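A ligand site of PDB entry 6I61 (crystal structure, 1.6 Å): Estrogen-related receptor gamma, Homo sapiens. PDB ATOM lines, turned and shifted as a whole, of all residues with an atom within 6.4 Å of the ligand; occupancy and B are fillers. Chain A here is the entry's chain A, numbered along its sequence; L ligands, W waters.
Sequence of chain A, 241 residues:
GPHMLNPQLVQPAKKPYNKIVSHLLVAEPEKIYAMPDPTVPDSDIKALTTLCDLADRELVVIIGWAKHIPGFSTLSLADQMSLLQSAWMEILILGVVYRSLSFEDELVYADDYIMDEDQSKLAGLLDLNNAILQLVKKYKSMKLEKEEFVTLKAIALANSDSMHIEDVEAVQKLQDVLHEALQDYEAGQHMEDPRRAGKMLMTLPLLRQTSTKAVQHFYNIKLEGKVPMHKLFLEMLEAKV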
ATOM      1  N   LEU A  48     -10.061  33.181   3.213  1.00  0.00           N
ATOM      2  CA  LEU A  48     -10.462  32.066   2.371  1.00  0.00           C
ATOM      3  C   LEU A  48      -9.367  31.014   2.272  1.00  0.00           C
ATOM      4  O   LEU A  48      -9.646  29.810   2.259  1.00  0.00           O
ATOM      5  CB  LEU A  48     -10.859  32.571   0.979  1.00  0.00           C
ATOM      6  CG  LEU A  48     -12.086  33.476   1.015  1.00  0.00           C
ATOM      7  CD1 LEU A  48     -12.255  34.135  -0.352  1.00  0.00           C
ATOM      8  CD2 LEU A  48     -13.358  32.691   1.388  1.00  0.00           C
ATOM      9  N   LEU A  51      -9.431  29.068   5.515  1.00  0.00           N
ATOM     10  CA  LEU A  51     -10.608  28.197   5.608  1.00  0.00           C
ATOM     11  C   LEU A  51     -10.486  26.976   4.717  1.00  0.00           C
ATOM     12  O   LEU A  51     -10.848  25.863   5.116  1.00  0.00           O
ATOM     13  CB  LEU A  51     -11.861  28.988   5.269  1.00  0.00           C
ATOM     14  CG  LEU A  51     -12.365  29.940   6.343  1.00  0.00           C
ATOM     15  CD1 LEU A  51     -13.472  30.802   5.768  1.00  0.00           C
ATOM     16  CD2 LEU A  51     -12.853  29.209   7.588  1.00  0.00           C
ATOM     17  N   CYS A  52     -10.017  27.159   3.479  1.00  0.00           N
ATOM     18  CA  CYS A  52      -9.882  25.994   2.596  1.00  0.00           C
ATOM     19  C   CYS A  52      -8.751  25.091   3.040  1.00  0.00           C
ATOM     20  O   CYS A  52      -8.796  23.883   2.800  1.00  0.00           O
ATOM     21  CB  CYS A  52      -9.664  26.445   1.145  1.00  0.00           C
ATOM     22  SG  CYS A  52     -11.073  27.307   0.456  1.00  0.00           S
ATOM     23  N   LEU A  54      -7.978  24.588   6.242  1.00  0.00           N
ATOM     24  CA  LEU A  54      -8.577  23.852   7.354  1.00  0.00           C
ATOM     25  C   LEU A  54      -9.462  22.743   6.805  1.00  0.00           C
ATOM     26  O   LEU A  54      -9.398  21.596   7.279  1.00  0.00           O
ATOM     27  CB  LEU A  54      -9.392  24.804   8.224  1.00  0.00           C
ATOM     28  CG  LEU A  54     -10.251  24.199   9.324  1.00  0.00           C
ATOM     29  CD1 LEU A  54      -9.356  23.578  10.401  1.00  0.00           C
ATOM     30  CD2 LEU A  54     -11.184  25.246   9.937  1.00  0.00           C
ATOM     31  N   ALA A  55     -10.281  23.071   5.801  1.00  0.00           N
ATOM     32  CA  ALA A  55     -11.186  22.069   5.212  1.00  0.00           C
ATOM     33  C   ALA A  55     -10.403  20.901   4.632  1.00  0.00           C
ATOM     34  O   ALA A  55     -10.811  19.741   4.773  1.00  0.00           O
ATOM     35  CB  ALA A  55     -12.059  22.712   4.136  1.00  0.00           C
ATOM     36  N   GLU A  58      -9.381  18.729   7.453  1.00  0.00           N
ATOM     37  CA  GLU A  58     -10.544  18.045   8.028  1.00  0.00           C
ATOM     38  C   GLU A  58     -11.022  16.911   7.129  1.00  0.00           C
ATOM     39  O   GLU A  58     -11.547  15.911   7.625  1.00  0.00           O
ATOM     40  CB  GLU A  58     -11.690  19.022   8.262  1.00  0.00           C
ATOM     41  CG  GLU A  58     -11.457  20.014   9.394  1.00  0.00           C
ATOM     42  CD  GLU A  58     -12.741  20.709   9.765  1.00  0.00           C
ATOM     43  OE1 GLU A  58     -13.705  20.014  10.114  1.00  0.00           O
ATOM     44  OE2 GLU A  58     -12.814  21.945   9.675  1.00  0.00           O
ATOM     45  N   TRP A  88     -19.339  15.498   1.703  1.00  0.00           N
ATOM     46  CA  TRP A  88     -18.252  16.092   2.487  1.00  0.00           C
ATOM     47  C   TRP A  88     -18.612  17.482   2.993  1.00  0.00           C
ATOM     48  O   TRP A  88     -18.284  17.841   4.126  1.00  0.00           O
ATOM     49  CB  TRP A  88     -16.959  16.129   1.674  1.00  0.00           C
ATOM     50  CG  TRP A  88     -17.012  16.986   0.443  1.00  0.00           C
ATOM     51  CD1 TRP A  88     -17.470  16.607  -0.783  1.00  0.00           C
ATOM     52  CD2 TRP A  88     -16.573  18.354   0.306  1.00  0.00           C
ATOM     53  NE1 TRP A  88     -17.352  17.648  -1.672  1.00  0.00           N
ATOM     54  CE2 TRP A  88     -16.805  18.733  -1.023  1.00  0.00           C
ATOM     55  CE3 TRP A  88     -16.022  19.289   1.193  1.00  0.00           C
ATOM     56  CZ2 TRP A  88     -16.503  20.011  -1.509  1.00  0.00           C
ATOM     57  CZ3 TRP A  88     -15.713  20.544   0.711  1.00  0.00           C
ATOM     58  CH2 TRP A  88     -15.953  20.904  -0.630  1.00  0.00           C
ATOM     59  N   MET A  89     -19.287  18.289   2.161  1.00  0.00           N
ATOM     60  CA  MET A  89     -19.606  19.647   2.565  1.00  0.00           C
ATOM     61  C   MET A  89     -20.629  19.654   3.697  1.00  0.00           C
ATOM     62  O   MET A  89     -20.495  20.433   4.649  1.00  0.00           O
ATOM     63  CB  MET A  89     -20.096  20.454   1.369  1.00  0.00           C
ATOM     64  CG  MET A  89     -20.438  21.897   1.699  1.00  0.00           C
ATOM     65  SD  MET A  89     -18.982  22.903   2.102  1.00  0.00           S
ATOM     66  CE  MET A  89     -18.436  23.285   0.433  1.00  0.00           C
ATOM     67  N   LEU A  92     -18.691  18.801   6.897  1.00  0.00           N
ATOM     68  CA  LEU A  92     -17.918  19.942   7.391  1.00  0.00           C
ATOM     69  C   LEU A  92     -18.836  20.986   8.022  1.00  0.00           C
ATOM     70  O   LEU A  92     -18.530  21.514   9.096  1.00  0.00           O
ATOM     71  CB  LEU A  92     -17.114  20.575   6.251  1.00  0.00           C
ATOM     72  CG  LEU A  92     -15.944  19.767   5.708  1.00  0.00           C
ATOM     73  CD1 LEU A  92     -15.345  20.482   4.511  1.00  0.00           C
ATOM     74  CD2 LEU A  92     -14.887  19.618   6.792  1.00  0.00           C
ATOM     75  N   ILE A  93     -19.941  21.303   7.360  1.00  0.00           N
ATOM     76  CA  ILE A  93     -20.843  22.342   7.857  1.00  0.00           C
ATOM     77  C   ILE A  93     -21.507  21.910   9.161  1.00  0.00           C
ATOM     78  O   ILE A  93     -21.602  22.691  10.105  1.00  0.00           O
ATOM     79  CB  ILE A  93     -21.861  22.735   6.771  1.00  0.00           C
ATOM     80  CG1 ILE A  93     -21.133  23.526   5.677  1.00  0.00           C
ATOM     81  CG2 ILE A  93     -22.975  23.565   7.394  1.00  0.00           C
ATOM     82  CD1 ILE A  93     -22.009  23.817   4.437  1.00  0.00           C
ATOM     83  N   GLY A  95     -20.196  20.149  11.364  1.00  0.00           N
ATOM     84  CA  GLY A  95     -19.152  20.345  12.368  1.00  0.00           C
ATOM     85  C   GLY A  95     -19.084  21.773  12.900  1.00  0.00           C
ATOM     86  O   GLY A  95     -19.114  21.989  14.114  1.00  0.00           O
ATOM     87  N   VAL A  96     -18.972  22.763  12.013  1.00  0.00           N
ATOM     88  CA  VAL A  96     -18.899  24.134  12.504  1.00  0.00           C
ATOM     89  C   VAL A  96     -20.196  24.504  13.206  1.00  0.00           C
ATOM     90  O   VAL A  96     -20.168  25.214  14.227  1.00  0.00           O
ATOM     91  CB  VAL A  96     -18.518  25.115  11.386  1.00  0.00           C
ATOM     92  CG1 VAL A  96     -19.543  25.139  10.235  1.00  0.00           C
ATOM     93  CG2 VAL A  96     -18.297  26.530  11.951  1.00  0.00           C
ATOM     94  N   ARG A  99     -19.931  23.114  16.719  1.00  0.00           N
ATOM     95  CA  ARG A  99     -18.958  23.833  17.527  1.00  0.00           C
ATOM     96  C   ARG A  99     -19.450  25.222  17.913  1.00  0.00           C
ATOM     97  O   ARG A  99     -18.916  25.815  18.864  1.00  0.00           O
ATOM     98  CB  ARG A  99     -17.639  23.952  16.777  1.00  0.00           C
ATOM     99  CG  ARG A  99     -16.988  22.608  16.505  1.00  0.00           C
ATOM    100  CD  ARG A  99     -15.587  22.772  15.949  1.00  0.00           C
ATOM    101  NE  ARG A  99     -15.518  23.361  14.608  1.00  0.00           N
ATOM    102  CZ  ARG A  99     -15.663  22.663  13.478  1.00  0.00           C
ATOM    103  NH1 ARG A  99     -15.927  21.355  13.527  1.00  0.00           N
ATOM    104  NH2 ARG A  99     -15.514  23.259  12.304  1.00  0.00           N
ATOM    105  N   LEU A 107     -19.270  31.912  14.285  1.00  0.00           N
ATOM    106  CA  LEU A 107     -19.060  30.558  13.780  1.00  0.00           C
ATOM    107  C   LEU A 107     -17.665  30.073  14.170  1.00  0.00           C
ATOM    108  O   LEU A 107     -16.660  30.700  13.795  1.00  0.00           O
ATOM    109  CB  LEU A 107     -19.245  30.523  12.272  1.00  0.00           C
ATOM    110  CG  LEU A 107     -20.683  30.758  11.831  1.00  0.00           C
ATOM    111  CD1 LEU A 107     -20.704  30.758  10.334  1.00  0.00           C
ATOM    112  CD2 LEU A 107     -21.626  29.660  12.392  1.00  0.00           C
ATOM    113  N   VAL A 108     -17.612  28.960  14.896  1.00  0.00           N
ATOM    114  CA  VAL A 108     -16.350  28.438  15.455  1.00  0.00           C
ATOM    115  C   VAL A 108     -15.817  27.425  14.448  1.00  0.00           C
ATOM    116  O   VAL A 108     -15.997  26.210  14.577  1.00  0.00           O
ATOM    117  CB  VAL A 108     -16.563  27.832  16.848  1.00  0.00           C
ATOM    118  CG1 VAL A 108     -15.242  27.238  17.410  1.00  0.00           C
ATOM    119  CG2 VAL A 108     -17.158  28.855  17.802  1.00  0.00           C
ATOM    120  N   TYR A 109     -15.120  27.931  13.419  1.00  0.00           N
ATOM    121  CA  TYR A 109     -14.498  27.021  12.473  1.00  0.00           C
ATOM    122  C   TYR A 109     -13.404  26.206  13.150  1.00  0.00           C
ATOM    123  O   TYR A 109     -13.228  25.025  12.842  1.00  0.00           O
ATOM    124  CB  TYR A 109     -13.973  27.798  11.253  1.00  0.00           C
ATOM    125  CG  TYR A 109     -15.117  28.201  10.355  1.00  0.00           C
ATOM    126  CD1 TYR A 109     -15.617  27.305   9.409  1.00  0.00           C
ATOM    127  CD2 TYR A 109     -15.737  29.442  10.482  1.00  0.00           C
ATOM    128  CE1 TYR A 109     -16.700  27.625   8.612  1.00  0.00           C
ATOM    129  CE2 TYR A 109     -16.836  29.767   9.658  1.00  0.00           C
ATOM    130  CZ  TYR A 109     -17.306  28.853   8.736  1.00  0.00           C
ATOM    131  OH  TYR A 109     -18.381  29.152   7.935  1.00  0.00           O
ATOM    132  N   MET A 115     -15.433  33.275  13.488  1.00  0.00           N
ATOM    133  CA  MET A 115     -15.817  34.351  12.563  1.00  0.00           C
ATOM    134  C   MET A 115     -17.081  35.044  13.065  1.00  0.00           C
ATOM    135  O   MET A 115     -18.116  34.391  13.265  1.00  0.00           O
ATOM    136  CB  MET A 115     -16.047  33.818  11.155  1.00  0.00           C
ATOM    137  CG  MET A 115     -14.808  33.248  10.484  1.00  0.00           C
ATOM    138  SD  MET A 115     -15.108  32.879   8.754  1.00  0.00           S
ATOM    139  CE  MET A 115     -15.221  34.542   8.081  1.00  0.00           C
ATOM    140  N   LEU A 125     -18.387  36.141   2.694  1.00  0.00           N
ATOM    141  CA  LEU A 125     -19.166  34.989   3.117  1.00  0.00           C
ATOM    142  C   LEU A 125     -20.378  35.362   3.965  1.00  0.00           C
ATOM    143  O   LEU A 125     -20.889  34.525   4.714  1.00  0.00           O
ATOM    144  CB  LEU A 125     -18.279  34.004   3.897  1.00  0.00           C
ATOM    145  CG  LEU A 125     -17.140  33.329   3.125  1.00  0.00           C
ATOM    146  CD1 LEU A 125     -16.164  32.636   4.081  1.00  0.00           C
ATOM    147  CD2 LEU A 125     -17.682  32.369   2.100  1.00  0.00           C
ATOM    148  N   LEU A 128     -23.566  33.278   3.071  1.00  0.00           N
ATOM    149  CA  LEU A 128     -23.375  31.854   3.331  1.00  0.00           C
ATOM    150  C   LEU A 128     -23.236  31.583   4.820  1.00  0.00           C
ATOM    151  O   LEU A 128     -23.852  30.642   5.346  1.00  0.00           O
ATOM    152  CB  LEU A 128     -22.154  31.381   2.556  1.00  0.00           C
ATOM    153  CG  LEU A 128     -21.925  29.909   2.232  1.00  0.00           C
ATOM    154  CD1 LEU A 128     -23.169  29.291   1.581  1.00  0.00           C
ATOM    155  CD2 LEU A 128     -20.728  29.840   1.287  1.00  0.00           C
ATOM    156  N   ASN A 129     -22.465  32.398   5.532  1.00  0.00           N
ATOM    157  CA  ASN A 129     -22.340  32.200   6.974  1.00  0.00           C
ATOM    158  C   ASN A 129     -23.633  32.508   7.706  1.00  0.00           C
ATOM    159  O   ASN A 129     -23.921  31.906   8.750  1.00  0.00           O
ATOM    160  CB  ASN A 129     -21.182  33.055   7.502  1.00  0.00           C
ATOM    161  CG  ASN A 129     -19.843  32.359   7.340  1.00  0.00           C
ATOM    162  OD1 ASN A 129     -19.768  31.220   6.876  1.00  0.00           O
ATOM    163  ND2 ASN A 129     -18.761  33.047   7.713  1.00  0.00           N
ATOM    164  N   ILE A 132     -25.499  29.331   7.591  1.00  0.00           N
ATOM    165  CA  ILE A 132     -24.989  28.432   8.616  1.00  0.00           C
ATOM    166  C   ILE A 132     -25.491  28.862   9.996  1.00  0.00           C
ATOM    167  O   ILE A 132     -25.839  28.026  10.821  1.00  0.00           O
ATOM    168  CB  ILE A 132     -23.453  28.366   8.546  1.00  0.00           C
ATOM    169  CG1 ILE A 132     -23.039  27.781   7.188  1.00  0.00           C
ATOM    170  CG2 ILE A 132     -22.870  27.499   9.672  1.00  0.00           C
ATOM    171  CD1 ILE A 132     -21.555  27.856   6.893  1.00  0.00           C
ATOM    172  N   ALA A 214     -22.858  26.411  -0.683  1.00  0.00           N
ATOM    173  CA  ALA A 214     -21.443  26.503  -0.346  1.00  0.00           C
ATOM    174  C   ALA A 214     -20.577  25.887  -1.448  1.00  0.00           C
ATOM    175  O   ALA A 214     -19.542  26.455  -1.816  1.00  0.00           O
ATOM    176  CB  ALA A 214     -21.169  25.827   0.997  1.00  0.00           C
ATOM    177  N   PHE A 218     -17.689  28.059  -3.407  1.00  0.00           N
ATOM    178  CA  PHE A 218     -16.256  27.765  -3.405  1.00  0.00           C
ATOM    179  C   PHE A 218     -15.775  27.211  -4.733  1.00  0.00           C
ATOM    180  O   PHE A 218     -14.576  27.300  -5.029  1.00  0.00           O
ATOM    181  CB  PHE A 218     -15.909  26.833  -2.237  1.00  0.00           C
ATOM    182  CG  PHE A 218     -15.799  27.566  -0.944  1.00  0.00           C
ATOM    183  CD1 PHE A 218     -14.585  28.107  -0.549  1.00  0.00           C
ATOM    184  CD2 PHE A 218     -16.924  27.818  -0.178  1.00  0.00           C
ATOM    185  CE1 PHE A 218     -14.480  28.829   0.609  1.00  0.00           C
ATOM    186  CE2 PHE A 218     -16.833  28.551   0.994  1.00  0.00           C
ATOM    187  CZ  PHE A 218     -15.605  29.064   1.383  1.00  0.00           C
ATOM    188  N   PHE A 233      -8.968  18.864  -1.133  1.00  0.00           N
ATOM    189  CA  PHE A 233     -10.087  19.813  -1.223  1.00  0.00           C
ATOM    190  C   PHE A 233     -10.498  20.027  -2.675  1.00  0.00           C
ATOM    191  O   PHE A 233     -11.692  20.052  -2.983  1.00  0.00           O
ATOM    192  CB  PHE A 233      -9.690  21.130  -0.549  1.00  0.00           C
ATOM    193  CG  PHE A 233     -10.784  22.170  -0.503  1.00  0.00           C
ATOM    194  CD1 PHE A 233     -11.778  22.106   0.461  1.00  0.00           C
ATOM    195  CD2 PHE A 233     -10.802  23.234  -1.404  1.00  0.00           C
ATOM    196  CE1 PHE A 233     -12.775  23.062   0.534  1.00  0.00           C
ATOM    197  CE2 PHE A 233     -11.815  24.193  -1.349  1.00  0.00           C
ATOM    198  CZ  PHE A 233     -12.801  24.106  -0.371  1.00  0.00           C
HETATM  199  C1  LIG L   1     -15.669  25.020   1.918  1.00  0.00           C
HETATM  200  C2  LIG L   1     -14.231  26.357   4.065  1.00  0.00           C
HETATM  201  C3  LIG L   1     -18.878  27.381   3.946  1.00  0.00           C
HETATM  202  C4  LIG L   1     -17.353  28.839   5.085  1.00  0.00           C
HETATM  203  C5  LIG L   1     -14.010  24.126   7.495  1.00  0.00           C
HETATM  204  C6  LIG L   1     -16.414  23.911   7.569  1.00  0.00           C
HETATM  205  C7  LIG L   1     -17.877  26.404   3.909  1.00  0.00           C
HETATM  206  C8  LIG L   1     -16.353  27.863   5.039  1.00  0.00           C
HETATM  207  C9  LIG L   1     -14.144  24.780   6.277  1.00  0.00           C
HETATM  208  C10 LIG L   1     -16.533  24.563   6.360  1.00  0.00           C
HETATM  209  C11 LIG L   1     -15.700  24.525   3.374  1.00  0.00           C
HETATM  210  C12 LIG L   1     -18.608  28.604   4.544  1.00  0.00           C
HETATM  211  C13 LIG L   1     -15.161  23.691   8.163  1.00  0.00           C
HETATM  212  C14 LIG L   1     -16.601  26.619   4.445  1.00  0.00           C
HETATM  213  C15 LIG L   1     -15.404  25.006   5.685  1.00  0.00           C
HETATM  214  C16 LIG L   1     -15.548  25.644   4.435  1.00  0.00           C
HETATM  215  O1  LIG L   1     -19.571  29.571   4.595  1.00  0.00           O
HETATM  216  O2  LIG L   1     -15.078  23.033   9.365  1.00  0.00           O
HETATM  217  O   HOH W   1     -16.236  20.524  10.635  1.00  0.00           O
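Water W1 lies within hydrogen-bond range of OE1 of Glu 58 (2.6 Å), O of Leu 92 (2.9 Å), NH1 of Arg 99 (3.0 Å) and O2 of the ligand (3.0 Å).
The guanidinium group (NH2) of Arg 99 sits at hydrogen-bond distance from an oxygen (O2) of the ligand (3.0 Å). The side-chain carboxylate of Glu 58 lies within hydrogen-bond range of an oxygen (O2) of the ligand (2.5 Å). OD1 of Asn 129 is in hydrogen-bond range of O1 of the ligand (2.8 Å).
Residues that only touch the ligand: Leu 51 (3.6 Å), Leu 54 (3.9 Å), Ala 55 (3.6 Å), Met 89 (3.6 Å), Leu 92 (3.5 Å), Tyr 109 (3.0 Å), Leu 128 (3.4 Å), Ile 132 (3.5 Å), Phe 218 (3.7 Å) and Phe 233 (3.8 Å). Hydrophobic or aromatic side chains within 4 Å of the ligand: Leu 51, Leu 54, Ala 55, Met 89, Leu 92, Tyr 109, Leu 128, Ile 132, Phe 218 and Phe 233. Of the 24 residues printed, 13 come within 4 Å of the ligand. The nearest printed residue that does not touch the ligand is Ala 214 (4.04 Å).
The guanidinium group of Arg 99 sits close to the backbone carbonyl oxygen of Gly 95, 3.3 Å away. The backbone carbonyl oxygen (O) of Tyr 109 is in hydrogen-bond range of the guanidinium group (NH2) of Arg 99. The guanidinium group (NH2) of Arg 99 is in salt-bridge range of the side-chain carboxylate (OE2) of Glu 58, 3.99 Å away. NE of Arg 99 lies within hydrogen-bond range of O of Val 108 (2.9 Å). The side-chain amide oxygen (OD1) of Asn 129 lies within hydrogen-bond range of the side-chain hydroxyl (OH) of Tyr 109 (2.7 Å).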
